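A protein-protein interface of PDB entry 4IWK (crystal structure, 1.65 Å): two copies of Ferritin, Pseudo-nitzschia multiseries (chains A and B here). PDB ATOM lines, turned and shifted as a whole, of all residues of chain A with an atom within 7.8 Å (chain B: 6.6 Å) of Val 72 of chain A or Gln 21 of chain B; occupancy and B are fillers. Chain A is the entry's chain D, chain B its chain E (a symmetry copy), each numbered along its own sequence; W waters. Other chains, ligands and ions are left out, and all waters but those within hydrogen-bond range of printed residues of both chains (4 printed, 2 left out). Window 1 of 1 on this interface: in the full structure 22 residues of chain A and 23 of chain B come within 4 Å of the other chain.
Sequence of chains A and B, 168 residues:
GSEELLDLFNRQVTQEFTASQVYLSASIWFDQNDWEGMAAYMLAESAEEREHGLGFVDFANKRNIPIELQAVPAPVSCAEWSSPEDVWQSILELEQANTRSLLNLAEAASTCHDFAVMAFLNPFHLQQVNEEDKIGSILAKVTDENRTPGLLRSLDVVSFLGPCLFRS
The side-chain hydroxyl (OG) of Ser 46 of chain B sits at hydrogen-bond distance from the guanidinium group (NH2) of Arg 50 of chain A (2.9 Å).
N of Val 72 of chain B sits at hydrogen-bond distance from O of Val 72 of chain A (2.8 Å).
The side-chain hydroxyl (OG) of Ser 25 of chain B sits at hydrogen-bond distance from the backbone carbonyl oxygen (O) of Val 22 of chain B (2.6 Å).
The side-chain hydroxyl (OG) of Ser 20 of chain B is in hydrogen-bond range of the backbone carbonyl oxygen (O) of Ser 46 of chain B, at 2.7 Å.
Among the printed residues, merely in contact across the chains: Phe 17 of chain A with Leu 24 of chain B (3.6 Å), Gln 21 of chain A with Phe 17 of chain B (3.9 Å), Arg 50 of chain A with Ser 20 of chain B (3.99 Å), Leu 54 of chain A with Leu 24 of chain B (3.6 Å), Leu 69 of chain A with Gln 21 of chain B (3.7 Å), Leu 69 of chain A with Leu 24 of chain B (3.8 Å), Leu 69 of chain A with Ser 25 of chain B (3.7 Å), Leu 69 of chain A with Ile 28 of chain B (3.8 Å), Leu 69 of chain A with Ala 74 of chain B (3.7 Å), Leu 69 of chain A with Pro 75 of chain B (3.9 Å), Gln 70 of chain A with Ala 74 of chain B (3.9 Å), Ala 71 of chain A with Val 72 of chain B (3.3 Å), Ala 71 of chain A with Ala 74 of chain B (3.7 Å), Val 72 of chain A with Gln 21 of chain B (3.9 Å), Val 72 of chain A with Ala 71 of chain B (3.3 Å), Ala 74 of chain A with Gln 70 of chain B (3.8 Å) and Ala 74 of chain A with Ala 71 of chain B (3.7 Å).
Val 72 of chain A touches just these residues of chain B: Gln 21, Ala 71 and Val 72.
Gln 21 of chain B touches two residues of chain A.
Printed residues of chain A within 4 Å of Ser 20 of chain B: Arg 50.
Printed residues of chain A within 4 Å of Ala 74 of chain B: Leu 69 (3.7 Å), Gln 70 (3.9 Å) and Ala 71 (3.7 Å).
Of the printed residues of chain B, Leu 69 of chain A touches Gln 21, Leu 24, Ser 25, Ile 28, Ala 74 and Pro 75.
Thr 14 of chain A touches none of the printed residues of chain B.
The nearest residue of chain B that does not touch Val 72 of chain A is Gln 70 of chain B (4.6 Å).
The nearest residue of chain A that does not touch Gln 21 of chain B is Gln 70 of chain A (4.1 Å).
Hydrophobic or aromatic side chains of chain A that line the printed part of chain B: Phe 17, Leu 54, Leu 69, Ala 71, Val 72 and Ala 74.
Of the 20 printed residues of chain B, 12 touch a printed residue of chain A.
Printed residues of chain B that touch a printed residue of chain A: Phe 17, Ser 20, Gln 21, Leu 24, Ser 25, Ile 28, Ser 46, Gln 70, Ala 71, Val 72, Ala 74 and Pro 75.
Along chain B the printed residues that touch a printed residue of chain A span positions 17 to 75.
Among the printed residues, no Asp or Glu carboxylate lies within 4 Å of a Lys or Arg side-chain nitrogen of the other chain.
Gln 70 of chain A touches Ala 74 of chain B, and with the chains exchanged Ala 74 of chain A touches Gln 70 of chain B.
Ala 71 of chain A touches Ala 74 of chain B, and with the chains exchanged Ala 74 of chain A touches Ala 71 of chain B.
Of the 19 pairs that touch across the chains among the printed residues, 7 have their exchanged pair printed and touching as well.
Water W1 lies within hydrogen-bond range of OE1 of Gln 21 of chain B (2.8 Å), OG of Ser 20 of chain B (2.9 Å), OG of Ser 46 of chain B (3.1 Å) and NE of Arg 50 of chain A (3.4 Å).
Water W2 bridges the backbone carbonyl oxygen (O) of Gln 70 of chain A (2.9 Å) and the side-chain amide nitrogen (NE2) of Gln 21 of chain B (3.0 Å).
Water W4 lies within hydrogen-bond range of O of Gln 70 of chain B (2.9 Å) and NE2 of Gln 21 of chain A (3.1 Å).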
ATOM      1  N   VAL A  13      -9.083 -15.800   4.281  1.00  0.00           N
ATOM      2  CA  VAL A  13      -9.060 -14.328   3.991  1.00  0.00           C
ATOM      3  C   VAL A  13     -10.063 -14.001   2.891  1.00  0.00           C
ATOM      4  O   VAL A  13     -10.868 -13.057   2.961  1.00  0.00           O
ATOM      5  CB  VAL A  13      -7.667 -13.865   3.594  1.00  0.00           C
ATOM      6  CG1 VAL A  13      -7.613 -12.434   3.140  1.00  0.00           C
ATOM      7  CG2 VAL A  13      -6.725 -14.155   4.800  1.00  0.00           C
ATOM      8  N   THR A  14     -10.075 -14.852   1.880  1.00  0.00           N
ATOM      9  CA  THR A  14     -11.007 -14.573   0.754  1.00  0.00           C
ATOM     10  C   THR A  14     -12.452 -14.657   1.244  1.00  0.00           C
ATOM     11  O   THR A  14     -13.269 -13.870   0.762  1.00  0.00           O
ATOM     12  CB  THR A  14     -10.778 -15.609  -0.316  1.00  0.00           C
ATOM     13  OG1 THR A  14      -9.376 -15.548  -0.708  1.00  0.00           O
ATOM     14  CG2 THR A  14     -11.692 -15.339  -1.607  1.00  0.00           C
ATOM     15  N   GLN A  15     -12.736 -15.695   2.075  1.00  0.00           N
ATOM     16  CA  GLN A  15     -14.075 -15.790   2.562  1.00  0.00           C
ATOM     17  C   GLN A  15     -14.549 -14.563   3.318  1.00  0.00           C
ATOM     18  O   GLN A  15     -15.691 -14.082   3.180  1.00  0.00           O
ATOM     19  CB  GLN A  15     -14.172 -17.050   3.447  1.00  0.00           C
ATOM     20  CG  GLN A  15     -15.581 -17.292   4.009  1.00  0.00           C
ATOM     21  CD  GLN A  15     -16.699 -17.506   2.940  1.00  0.00           C
ATOM     22  OE1 GLN A  15     -16.456 -18.020   1.841  1.00  0.00           O
ATOM     23  NE2 GLN A  15     -17.876 -17.032   3.248  1.00  0.00           N
ATOM     24  N   GLU A  16     -13.678 -14.080   4.233  1.00  0.00           N
ATOM     25  CA  GLU A  16     -14.043 -12.893   5.014  1.00  0.00           C
ATOM     26  C   GLU A  16     -14.249 -11.677   4.061  1.00  0.00           C
ATOM     27  O   GLU A  16     -15.221 -10.936   4.326  1.00  0.00           O
ATOM     28  CB  GLU A  16     -12.990 -12.494   6.044  1.00  0.00           C
ATOM     29  CG  GLU A  16     -12.701 -13.641   7.033  1.00  0.00           C
ATOM     30  CD  GLU A  16     -13.791 -14.027   7.998  1.00  0.00           C
ATOM     31  OE1 GLU A  16     -14.699 -13.245   8.115  1.00  0.00           O
ATOM     32  OE2 GLU A  16     -13.686 -15.122   8.646  1.00  0.00           O
ATOM     33  N   PHE A  17     -13.401 -11.512   3.043  1.00  0.00           N
ATOM     34  CA  PHE A  17     -13.593 -10.334   2.181  1.00  0.00           C
ATOM     35  C   PHE A  17     -14.850 -10.552   1.276  1.00  0.00           C
ATOM     36  O   PHE A  17     -15.525  -9.594   0.967  1.00  0.00           O
ATOM     37  CB  PHE A  17     -12.328 -10.113   1.360  1.00  0.00           C
ATOM     38  CG  PHE A  17     -11.171  -9.593   2.221  1.00  0.00           C
ATOM     39  CD1 PHE A  17     -11.304  -9.004   3.496  1.00  0.00           C
ATOM     40  CD2 PHE A  17      -9.913  -9.720   1.658  1.00  0.00           C
ATOM     41  CE1 PHE A  17     -10.155  -8.512   4.195  1.00  0.00           C
ATOM     42  CE2 PHE A  17      -8.787  -9.250   2.350  1.00  0.00           C
ATOM     43  CZ  PHE A  17      -8.927  -8.665   3.576  1.00  0.00           C
ATOM     44  N   THR A  18     -15.127 -11.824   0.905  1.00  0.00           N
ATOM     45  CA  THR A  18     -16.335 -12.113   0.115  1.00  0.00           C
ATOM     46  C   THR A  18     -17.547 -11.733   0.966  1.00  0.00           C
ATOM     47  O   THR A  18     -18.494 -11.113   0.511  1.00  0.00           O
ATOM     48  CB  THR A  18     -16.345 -13.611  -0.204  1.00  0.00           C
ATOM     49  OG1 THR A  18     -15.248 -13.818  -1.124  1.00  0.00           O
ATOM     50  CG2 THR A  18     -17.703 -13.973  -0.883  1.00  0.00           C
ATOM     51  N   ALA A  19     -17.473 -12.073   2.257  1.00  0.00           N
ATOM     52  CA  ALA A  19     -18.586 -11.747   3.124  1.00  0.00           C
ATOM     53  C   ALA A  19     -18.707 -10.249   3.340  1.00  0.00           C
ATOM     54  O   ALA A  19     -19.826  -9.745   3.374  1.00  0.00           O
ATOM     55  CB  ALA A  19     -18.404 -12.493   4.492  1.00  0.00           C
ATOM     56  N   SER A  20     -17.586  -9.521   3.426  1.00  0.00           N
ATOM     57  CA  SER A  20     -17.691  -8.078   3.553  1.00  0.00           C
ATOM     58  C   SER A  20     -18.423  -7.533   2.323  1.00  0.00           C
ATOM     59  O   SER A  20     -19.230  -6.665   2.455  1.00  0.00           O
ATOM     60  CB  SER A  20     -16.252  -7.538   3.638  1.00  0.00           C
ATOM     61  OG  SER A  20     -16.248  -6.104   3.634  1.00  0.00           O
ATOM     62  N   GLN A  21     -18.117  -8.039   1.135  1.00  0.00           N
ATOM     63  CA  GLN A  21     -18.840  -7.522  -0.085  1.00  0.00           C
ATOM     64  C   GLN A  21     -20.320  -7.897  -0.172  1.00  0.00           C
ATOM     65  O   GLN A  21     -21.188  -7.097  -0.603  1.00  0.00           O
ATOM     66  CB  GLN A  21     -18.124  -8.070  -1.355  1.00  0.00           C
ATOM     67  CG  GLN A  21     -16.790  -7.347  -1.519  1.00  0.00           C
ATOM     68  CD  GLN A  21     -16.989  -5.853  -1.945  1.00  0.00           C
ATOM     69  OE1 GLN A  21     -16.915  -4.993  -1.055  1.00  0.00           O
ATOM     70  NE2 GLN A  21     -17.092  -5.570  -3.279  1.00  0.00           N
ATOM     71  N   VAL A  22     -20.602  -9.119   0.297  1.00  0.00           N
ATOM     72  CA  VAL A  22     -22.095  -9.554   0.315  1.00  0.00           C
ATOM     73  C   VAL A  22     -22.818  -8.643   1.336  1.00  0.00           C
ATOM     74  O   VAL A  22     -23.944  -8.169   1.057  1.00  0.00           O
ATOM     75  CB  VAL A  22     -22.224 -11.005   0.734  1.00  0.00           C
ATOM     76  CG1 VAL A  22     -23.716 -11.316   0.913  1.00  0.00           C
ATOM     77  CG2 VAL A  22     -21.651 -11.828  -0.387  1.00  0.00           C
ATOM     78  N   ARG A  50     -14.417  -7.258   7.039  1.00  0.00           N
ATOM     79  CA  ARG A  50     -13.045  -6.862   6.526  1.00  0.00           C
ATOM     80  C   ARG A  50     -12.036  -6.933   7.704  1.00  0.00           C
ATOM     81  O   ARG A  50     -10.925  -7.457   7.497  1.00  0.00           O
ATOM     82  CB  ARG A  50     -13.164  -5.450   5.922  1.00  0.00           C
ATOM     83  CG  ARG A  50     -11.815  -4.983   5.426  1.00  0.00           C
ATOM     84  CD  ARG A  50     -12.006  -3.682   4.648  1.00  0.00           C
ATOM     85  NE  ARG A  50     -10.714  -3.385   3.903  1.00  0.00           N
ATOM     86  CZ  ARG A  50      -9.888  -2.660   4.579  1.00  0.00           C
ATOM     87  NH1 ARG A  50     -10.341  -2.251   5.727  1.00  0.00           N
ATOM     88  NH2 ARG A  50      -8.699  -2.374   4.136  1.00  0.00           N
ATOM     89  N   LEU A  54      -8.515  -8.912   7.838  1.00  0.00           N
ATOM     90  CA  LEU A  54      -7.190  -8.260   8.116  1.00  0.00           C
ATOM     91  C   LEU A  54      -6.545  -8.980   9.276  1.00  0.00           C
ATOM     92  O   LEU A  54      -5.310  -9.043   9.297  1.00  0.00           O
ATOM     93  CB  LEU A  54      -7.481  -6.830   8.459  1.00  0.00           C
ATOM     94  CG  LEU A  54      -7.913  -6.013   7.193  1.00  0.00           C
ATOM     95  CD1 LEU A  54      -8.207  -4.605   7.717  1.00  0.00           C
ATOM     96  CD2 LEU A  54      -6.857  -6.015   6.048  1.00  0.00           C
ATOM     97  N   LEU A  69      -3.417 -12.532  -2.158  1.00  0.00           N
ATOM     98  CA  LEU A  69      -4.838 -12.138  -2.199  1.00  0.00           C
ATOM     99  C   LEU A  69      -5.471 -12.595  -3.486  1.00  0.00           C
ATOM    100  O   LEU A  69      -4.889 -12.522  -4.594  1.00  0.00           O
ATOM    101  CB  LEU A  69      -4.989 -10.637  -2.160  1.00  0.00           C
ATOM    102  CG  LEU A  69      -4.484  -9.971  -0.819  1.00  0.00           C
ATOM    103  CD1 LEU A  69      -4.548  -8.437  -0.918  1.00  0.00           C
ATOM    104  CD2 LEU A  69      -5.333 -10.483   0.351  1.00  0.00           C
ATOM    105  N   GLN A  70      -6.681 -13.147  -3.283  1.00  0.00           N
ATOM    106  CA  GLN A  70      -7.495 -13.625  -4.380  1.00  0.00           C
ATOM    107  C   GLN A  70      -8.563 -12.649  -4.810  1.00  0.00           C
ATOM    108  O   GLN A  70      -8.795 -11.652  -4.120  1.00  0.00           O
ATOM    109  CB  GLN A  70      -8.088 -14.999  -4.039  1.00  0.00           C
ATOM    110  CG  GLN A  70      -6.971 -15.975  -3.681  1.00  0.00           C
ATOM    111  CD  GLN A  70      -6.066 -16.436  -4.935  1.00  0.00           C
ATOM    112  OE1 GLN A  70      -6.332 -16.195  -6.172  1.00  0.00           O
ATOM    113  NE2 GLN A  70      -4.919 -16.979  -4.593  1.00  0.00           N
ATOM    114  N   ALA A  71      -9.223 -12.962  -5.961  1.00  0.00           N
ATOM    115  CA  ALA A  71     -10.357 -12.048  -6.338  1.00  0.00           C
ATOM    116  C   ALA A  71     -11.450 -12.091  -5.268  1.00  0.00           C
ATOM    117  O   ALA A  71     -11.559 -13.165  -4.572  1.00  0.00           O
ATOM    118  CB  ALA A  71     -10.997 -12.672  -7.642  1.00  0.00           C
ATOM    119  N   VAL A  72     -12.151 -10.999  -5.180  1.00  0.00           N
ATOM    120  CA  VAL A  72     -13.396 -10.962  -4.298  1.00  0.00           C
ATOM    121  C   VAL A  72     -14.526 -11.011  -5.320  1.00  0.00           C
ATOM    122  O   VAL A  72     -14.723 -10.019  -6.024  1.00  0.00           O
ATOM    123  CB  VAL A  72     -13.391  -9.782  -3.435  1.00  0.00           C
ATOM    124  CG1 VAL A  72     -14.493 -10.043  -2.395  1.00  0.00           C
ATOM    125  CG2 VAL A  72     -12.004  -9.818  -2.632  1.00  0.00           C
ATOM    126  N   PRO A  73     -15.297 -12.128  -5.350  1.00  0.00           N
ATOM    127  CA  PRO A  73     -16.311 -12.240  -6.405  1.00  0.00           C
ATOM    128  C   PRO A  73     -17.422 -11.232  -6.262  1.00  0.00           C
ATOM    129  O   PRO A  73     -17.681 -10.657  -5.136  1.00  0.00           O
ATOM    130  CB  PRO A  73     -16.891 -13.640  -6.238  1.00  0.00           C
ATOM    131  CG  PRO A  73     -16.605 -14.002  -4.777  1.00  0.00           C
ATOM    132  CD  PRO A  73     -15.227 -13.308  -4.441  1.00  0.00           C
ATOM    133  N   ALA A  74     -18.106 -10.899  -7.374  1.00  0.00           N
ATOM    134  CA  ALA A  74     -19.273 -10.011  -7.314  1.00  0.00           C
ATOM    135  C   ALA A  74     -20.438 -10.681  -6.553  1.00  0.00           C
ATOM    136  O   ALA A  74     -20.762 -11.859  -6.787  1.00  0.00           O
ATOM    137  CB  ALA A  74     -19.785  -9.749  -8.761  1.00  0.00           C
ATOM    138  N   PRO A  75     -21.029  -9.977  -5.626  1.00  0.00           N
ATOM    139  CA  PRO A  75     -22.186 -10.598  -4.947  1.00  0.00           C
ATOM    140  C   PRO A  75     -23.347 -10.754  -5.949  1.00  0.00           C
ATOM    141  O   PRO A  75     -23.573  -9.818  -6.774  1.00  0.00           O
ATOM    142  CB  PRO A  75     -22.571  -9.516  -3.888  1.00  0.00           C
ATOM    143  CG  PRO A  75     -21.311  -8.830  -3.631  1.00  0.00           C
ATOM    144  CD  PRO A  75     -20.585  -8.743  -4.975  1.00  0.00           C
ATOM    145  N   GLU B  16     -12.032   2.137  -6.783  1.00  0.00           N
ATOM    146  CA  GLU B  16     -11.621   2.424  -5.367  1.00  0.00           C
ATOM    147  C   GLU B  16     -11.459   1.114  -4.630  1.00  0.00           C
ATOM    148  O   GLU B  16     -10.443   1.004  -3.895  1.00  0.00           O
ATOM    149  CB  GLU B  16     -12.735   3.196  -4.633  1.00  0.00           C
ATOM    150  CG  GLU B  16     -13.001   4.596  -5.314  1.00  0.00           C
ATOM    151  CD  GLU B  16     -11.860   5.624  -5.318  1.00  0.00           C
ATOM    152  OE1 GLU B  16     -10.899   5.368  -4.612  1.00  0.00           O
ATOM    153  OE2 GLU B  16     -11.942   6.690  -6.036  1.00  0.00           O
ATOM    154  N   PHE B  17     -12.367   0.110  -4.826  1.00  0.00           N
ATOM    155  CA  PHE B  17     -12.092  -1.142  -4.133  1.00  0.00           C
ATOM    156  C   PHE B  17     -10.923  -1.909  -4.679  1.00  0.00           C
ATOM    157  O   PHE B  17     -10.277  -2.600  -3.901  1.00  0.00           O
ATOM    158  CB  PHE B  17     -13.406  -1.992  -4.182  1.00  0.00           C
ATOM    159  CG  PHE B  17     -14.561  -1.396  -3.371  1.00  0.00           C
ATOM    160  CD1 PHE B  17     -14.404  -0.438  -2.358  1.00  0.00           C
ATOM    161  CD2 PHE B  17     -15.815  -1.886  -3.650  1.00  0.00           C
ATOM    162  CE1 PHE B  17     -15.476   0.051  -1.657  1.00  0.00           C
ATOM    163  CE2 PHE B  17     -16.944  -1.381  -2.981  1.00  0.00           C
ATOM    164  CZ  PHE B  17     -16.787  -0.438  -1.985  1.00  0.00           C
ATOM    165  N   THR B  18     -10.666  -1.839  -5.994  1.00  0.00           N
ATOM    166  CA  THR B  18      -9.462  -2.430  -6.570  1.00  0.00           C
ATOM    167  C   THR B  18      -8.249  -1.783  -5.896  1.00  0.00           C
ATOM    168  O   THR B  18      -7.324  -2.502  -5.472  1.00  0.00           O
ATOM    169  CB  THR B  18      -9.420  -2.219  -8.075  1.00  0.00           C
ATOM    170  OG1 THR B  18     -10.535  -2.977  -8.631  1.00  0.00           O
ATOM    171  CG2 THR B  18      -8.102  -2.757  -8.714  1.00  0.00           C
ATOM    172  N   ALA B  19      -8.292  -0.447  -5.806  1.00  0.00           N
ATOM    173  CA  ALA B  19      -7.130   0.234  -5.135  1.00  0.00           C
ATOM    174  C   ALA B  19      -6.999  -0.146  -3.695  1.00  0.00           C
ATOM    175  O   ALA B  19      -5.882  -0.370  -3.254  1.00  0.00           O
ATOM    176  CB  ALA B  19      -7.260   1.780  -5.265  1.00  0.00           C
ATOM    177  N   SER B  20      -8.106  -0.404  -2.982  1.00  0.00           N
ATOM    178  CA  SER B  20      -7.994  -0.820  -1.617  1.00  0.00           C
ATOM    179  C   SER B  20      -7.298  -2.192  -1.519  1.00  0.00           C
ATOM    180  O   SER B  20      -6.412  -2.441  -0.673  1.00  0.00           O
ATOM    181  CB  SER B  20      -9.410  -0.924  -1.015  1.00  0.00           C
ATOM    182  OG  SER B  20      -9.306  -1.418   0.312  1.00  0.00           O
ATOM    183  N   GLN B  21      -7.644  -3.069  -2.443  1.00  0.00           N
ATOM    184  CA  GLN B  21      -6.910  -4.384  -2.465  1.00  0.00           C
ATOM    185  C   GLN B  21      -5.438  -4.351  -2.863  1.00  0.00           C
ATOM    186  O   GLN B  21      -4.601  -5.051  -2.326  1.00  0.00           O
ATOM    187  CB  GLN B  21      -7.685  -5.283  -3.436  1.00  0.00           C
ATOM    188  CG  GLN B  21      -8.979  -5.775  -2.871  1.00  0.00           C
ATOM    189  CD  GLN B  21      -8.796  -6.782  -1.718  1.00  0.00           C
ATOM    190  OE1 GLN B  21      -8.862  -6.285  -0.577  1.00  0.00           O
ATOM    191  NE2 GLN B  21      -8.570  -8.137  -1.986  1.00  0.00           N
ATOM    192  N   VAL B  22      -5.133  -3.466  -3.835  1.00  0.00           N
ATOM    193  CA  VAL B  22      -3.724  -3.252  -4.264  1.00  0.00           C
ATOM    194  C   VAL B  22      -2.962  -2.692  -3.062  1.00  0.00           C
ATOM    195  O   VAL B  22      -1.825  -3.226  -2.767  1.00  0.00           O
ATOM    196  CB  VAL B  22      -3.641  -2.351  -5.467  1.00  0.00           C
ATOM    197  CG1 VAL B  22      -2.180  -2.135  -5.815  1.00  0.00           C
ATOM    198  CG2 VAL B  22      -4.288  -3.046  -6.694  1.00  0.00           C
ATOM    199  N   TYR B  23      -3.504  -1.740  -2.325  1.00  0.00           N
ATOM    200  CA  TYR B  23      -2.753  -1.266  -1.151  1.00  0.00           C
ATOM    201  C   TYR B  23      -2.586  -2.339  -0.136  1.00  0.00           C
ATOM    202  O   TYR B  23      -1.500  -2.459   0.486  1.00  0.00           O
ATOM    203  CB  TYR B  23      -3.524  -0.075  -0.492  1.00  0.00           C
ATOM    204  CG  TYR B  23      -3.149   1.262  -1.106  1.00  0.00           C
ATOM    205  CD1 TYR B  23      -4.060   2.048  -1.846  1.00  0.00           C
ATOM    206  CD2 TYR B  23      -1.908   1.838  -0.764  1.00  0.00           C
ATOM    207  CE1 TYR B  23      -3.687   3.276  -2.331  1.00  0.00           C
ATOM    208  CE2 TYR B  23      -1.522   3.115  -1.204  1.00  0.00           C
ATOM    209  CZ  TYR B  23      -2.429   3.822  -1.955  1.00  0.00           C
ATOM    210  OH  TYR B  23      -2.125   5.107  -2.378  1.00  0.00           O
ATOM    211  N   LEU B  24      -3.599  -3.256   0.067  1.00  0.00           N
ATOM    212  CA  LEU B  24      -3.391  -4.336   1.029  1.00  0.00           C
ATOM    213  C   LEU B  24      -2.297  -5.258   0.530  1.00  0.00           C
ATOM    214  O   LEU B  24      -1.481  -5.745   1.341  1.00  0.00           O
ATOM    215  CB  LEU B  24      -4.726  -5.066   1.180  1.00  0.00           C
ATOM    216  CG  LEU B  24      -4.626  -6.224   2.200  1.00  0.00           C
ATOM    217  CD1 LEU B  24      -4.331  -5.606   3.583  1.00  0.00           C
ATOM    218  CD2 LEU B  24      -6.042  -6.889   2.177  1.00  0.00           C
ATOM    219  N   SER B  25      -2.242  -5.519  -0.787  1.00  0.00           N
ATOM    220  CA  SER B  25      -1.157  -6.375  -1.252  1.00  0.00           C
ATOM    221  C   SER B  25       0.258  -5.765  -1.058  1.00  0.00           C
ATOM    222  O   SER B  25       1.172  -6.498  -0.721  1.00  0.00           O
ATOM    223  CB  SER B  25      -1.382  -6.640  -2.765  1.00  0.00           C
ATOM    224  OG  SER B  25      -1.006  -5.572  -3.654  1.00  0.00           O
ATOM    225  N   ALA B  26       0.308  -4.424  -1.114  1.00  0.00           N
ATOM    226  CA  ALA B  26       1.601  -3.703  -0.842  1.00  0.00           C
ATOM    227  C   ALA B  26       1.881  -3.859   0.651  1.00  0.00           C
ATOM    228  O   ALA B  26       3.074  -4.076   1.027  1.00  0.00           O
ATOM    229  CB  ALA B  26       1.468  -2.194  -1.261  1.00  0.00           C
ATOM    230  N   ILE B  28       1.093  -6.300   2.592  1.00  0.00           N
ATOM    231  CA  ILE B  28       1.585  -7.691   2.816  1.00  0.00           C
ATOM    232  C   ILE B  28       3.024  -7.877   2.325  1.00  0.00           C
ATOM    233  O   ILE B  28       3.903  -8.412   3.045  1.00  0.00           O
ATOM    234  CB  ILE B  28       0.673  -8.709   2.030  1.00  0.00           C
ATOM    235  CG1 ILE B  28      -0.646  -8.734   2.769  1.00  0.00           C
ATOM    236  CG2 ILE B  28       1.321 -10.076   1.969  1.00  0.00           C
ATOM    237  CD1 ILE B  28      -1.838  -9.287   1.881  1.00  0.00           C
ATOM    238  N   SER B  46      -5.224   1.394   2.411  1.00  0.00           N
ATOM    239  CA  SER B  46      -6.236   0.372   1.934  1.00  0.00           C
ATOM    240  C   SER B  46      -7.628   0.707   2.570  1.00  0.00           C
ATOM    241  O   SER B  46      -8.628   0.633   1.881  1.00  0.00           O
ATOM    242  CB  SER B  46      -5.772  -1.037   2.333  1.00  0.00           C
ATOM    243  OG  SER B  46      -6.788  -2.029   2.044  1.00  0.00           O
ATOM    244  N   GLU B  49      -9.032   3.894   0.849  1.00  0.00           N
ATOM    245  CA  GLU B  49      -9.622   3.717  -0.496  1.00  0.00           C
ATOM    246  C   GLU B  49     -10.989   3.039  -0.351  1.00  0.00           C
ATOM    247  O   GLU B  49     -11.972   3.364  -1.142  1.00  0.00           O
ATOM    248  CB  GLU B  49      -8.795   2.825  -1.390  1.00  0.00           C
ATOM    249  CG  GLU B  49      -7.424   3.486  -1.722  1.00  0.00           C
ATOM    250  CD  GLU B  49      -7.544   4.612  -2.678  1.00  0.00           C
ATOM    251  OE1 GLU B  49      -8.617   4.856  -3.161  1.00  0.00           O
ATOM    252  OE2 GLU B  49      -6.530   5.087  -3.136  1.00  0.00           O
ATOM    253  N   GLN B  70     -19.173  -5.083  -8.700  1.00  0.00           N
ATOM    254  CA  GLN B  70     -18.400  -5.955  -9.521  1.00  0.00           C
ATOM    255  C   GLN B  70     -17.390  -6.741  -8.709  1.00  0.00           C
ATOM    256  O   GLN B  70     -17.124  -6.464  -7.562  1.00  0.00           O
ATOM    257  CB  GLN B  70     -17.700  -5.140 -10.626  1.00  0.00           C
ATOM    258  CG  GLN B  70     -18.725  -4.477 -11.598  1.00  0.00           C
ATOM    259  CD  GLN B  70     -19.596  -5.537 -12.325  1.00  0.00           C
ATOM    260  OE1 GLN B  70     -19.168  -6.716 -12.538  1.00  0.00           O
ATOM    261  NE2 GLN B  70     -20.796  -5.146 -12.716  1.00  0.00           N
ATOM    262  N   ALA B  71     -16.800  -7.733  -9.358  1.00  0.00           N
ATOM    263  CA  ALA B  71     -15.732  -8.429  -8.695  1.00  0.00           C
ATOM    264  C   ALA B  71     -14.525  -7.527  -8.465  1.00  0.00           C
ATOM    265  O   ALA B  71     -14.340  -6.593  -9.289  1.00  0.00           O
ATOM    266  CB  ALA B  71     -15.242  -9.575  -9.667  1.00  0.00           C
ATOM    267  N   VAL B  72     -13.794  -7.781  -7.388  1.00  0.00           N
ATOM    268  CA  VAL B  72     -12.522  -6.971  -7.195  1.00  0.00           C
ATOM    269  C   VAL B  72     -11.428  -7.986  -7.623  1.00  0.00           C
ATOM    270  O   VAL B  72     -11.273  -8.994  -6.996  1.00  0.00           O
ATOM    271  CB  VAL B  72     -12.374  -6.566  -5.763  1.00  0.00           C
ATOM    272  CG1 VAL B  72     -11.150  -5.616  -5.675  1.00  0.00           C
ATOM    273  CG2 VAL B  72     -13.689  -5.829  -5.370  1.00  0.00           C
ATOM    274  N   PRO B  73     -10.677  -7.653  -8.690  1.00  0.00           N
ATOM    275  CA  PRO B  73      -9.743  -8.678  -9.245  1.00  0.00           C
ATOM    276  C   PRO B  73      -8.610  -8.935  -8.269  1.00  0.00           C
ATOM    277  O   PRO B  73      -8.272  -8.040  -7.428  1.00  0.00           O
ATOM    278  CB  PRO B  73      -9.231  -8.024 -10.503  1.00  0.00           C
ATOM    279  CG  PRO B  73      -9.303  -6.526 -10.257  1.00  0.00           C
ATOM    280  CD  PRO B  73     -10.601  -6.337  -9.444  1.00  0.00           C
ATOM    281  N   ALA B  74      -7.984 -10.100  -8.406  1.00  0.00           N
ATOM    282  CA  ALA B  74      -6.787 -10.450  -7.582  1.00  0.00           C
ATOM    283  C   ALA B  74      -5.690  -9.472  -7.953  1.00  0.00           C
ATOM    284  O   ALA B  74      -5.356  -9.255  -9.130  1.00  0.00           O
ATOM    285  CB  ALA B  74      -6.305 -11.828  -7.904  1.00  0.00           C
ATOM    286  N   PRO B  75      -5.019  -8.855  -6.969  1.00  0.00           N
ATOM    287  CA  PRO B  75      -3.859  -8.004  -7.330  1.00  0.00           C
ATOM    288  C   PRO B  75      -2.758  -8.847  -7.964  1.00  0.00           C
ATOM    289  O   PRO B  75      -2.583 -10.026  -7.612  1.00  0.00           O
ATOM    290  CB  PRO B  75      -3.401  -7.506  -5.925  1.00  0.00           C
ATOM    291  CG  PRO B  75      -4.668  -7.437  -5.061  1.00  0.00           C
ATOM    292  CD  PRO B  75      -5.436  -8.784  -5.545  1.00  0.00           C
HETATM  293  O   HOH W   1      -8.884  -4.126   1.169  1.00  0.00           O
HETATM  294  O   HOH W   2      -8.787 -11.056  -1.317  1.00  0.00           O
HETATM  295  O   HOH W   3      -2.521 -11.016  -4.969  1.00  0.00           O
HETATM  296  O   HOH W   4     -17.074  -4.060  -5.934  1.00  0.00           O
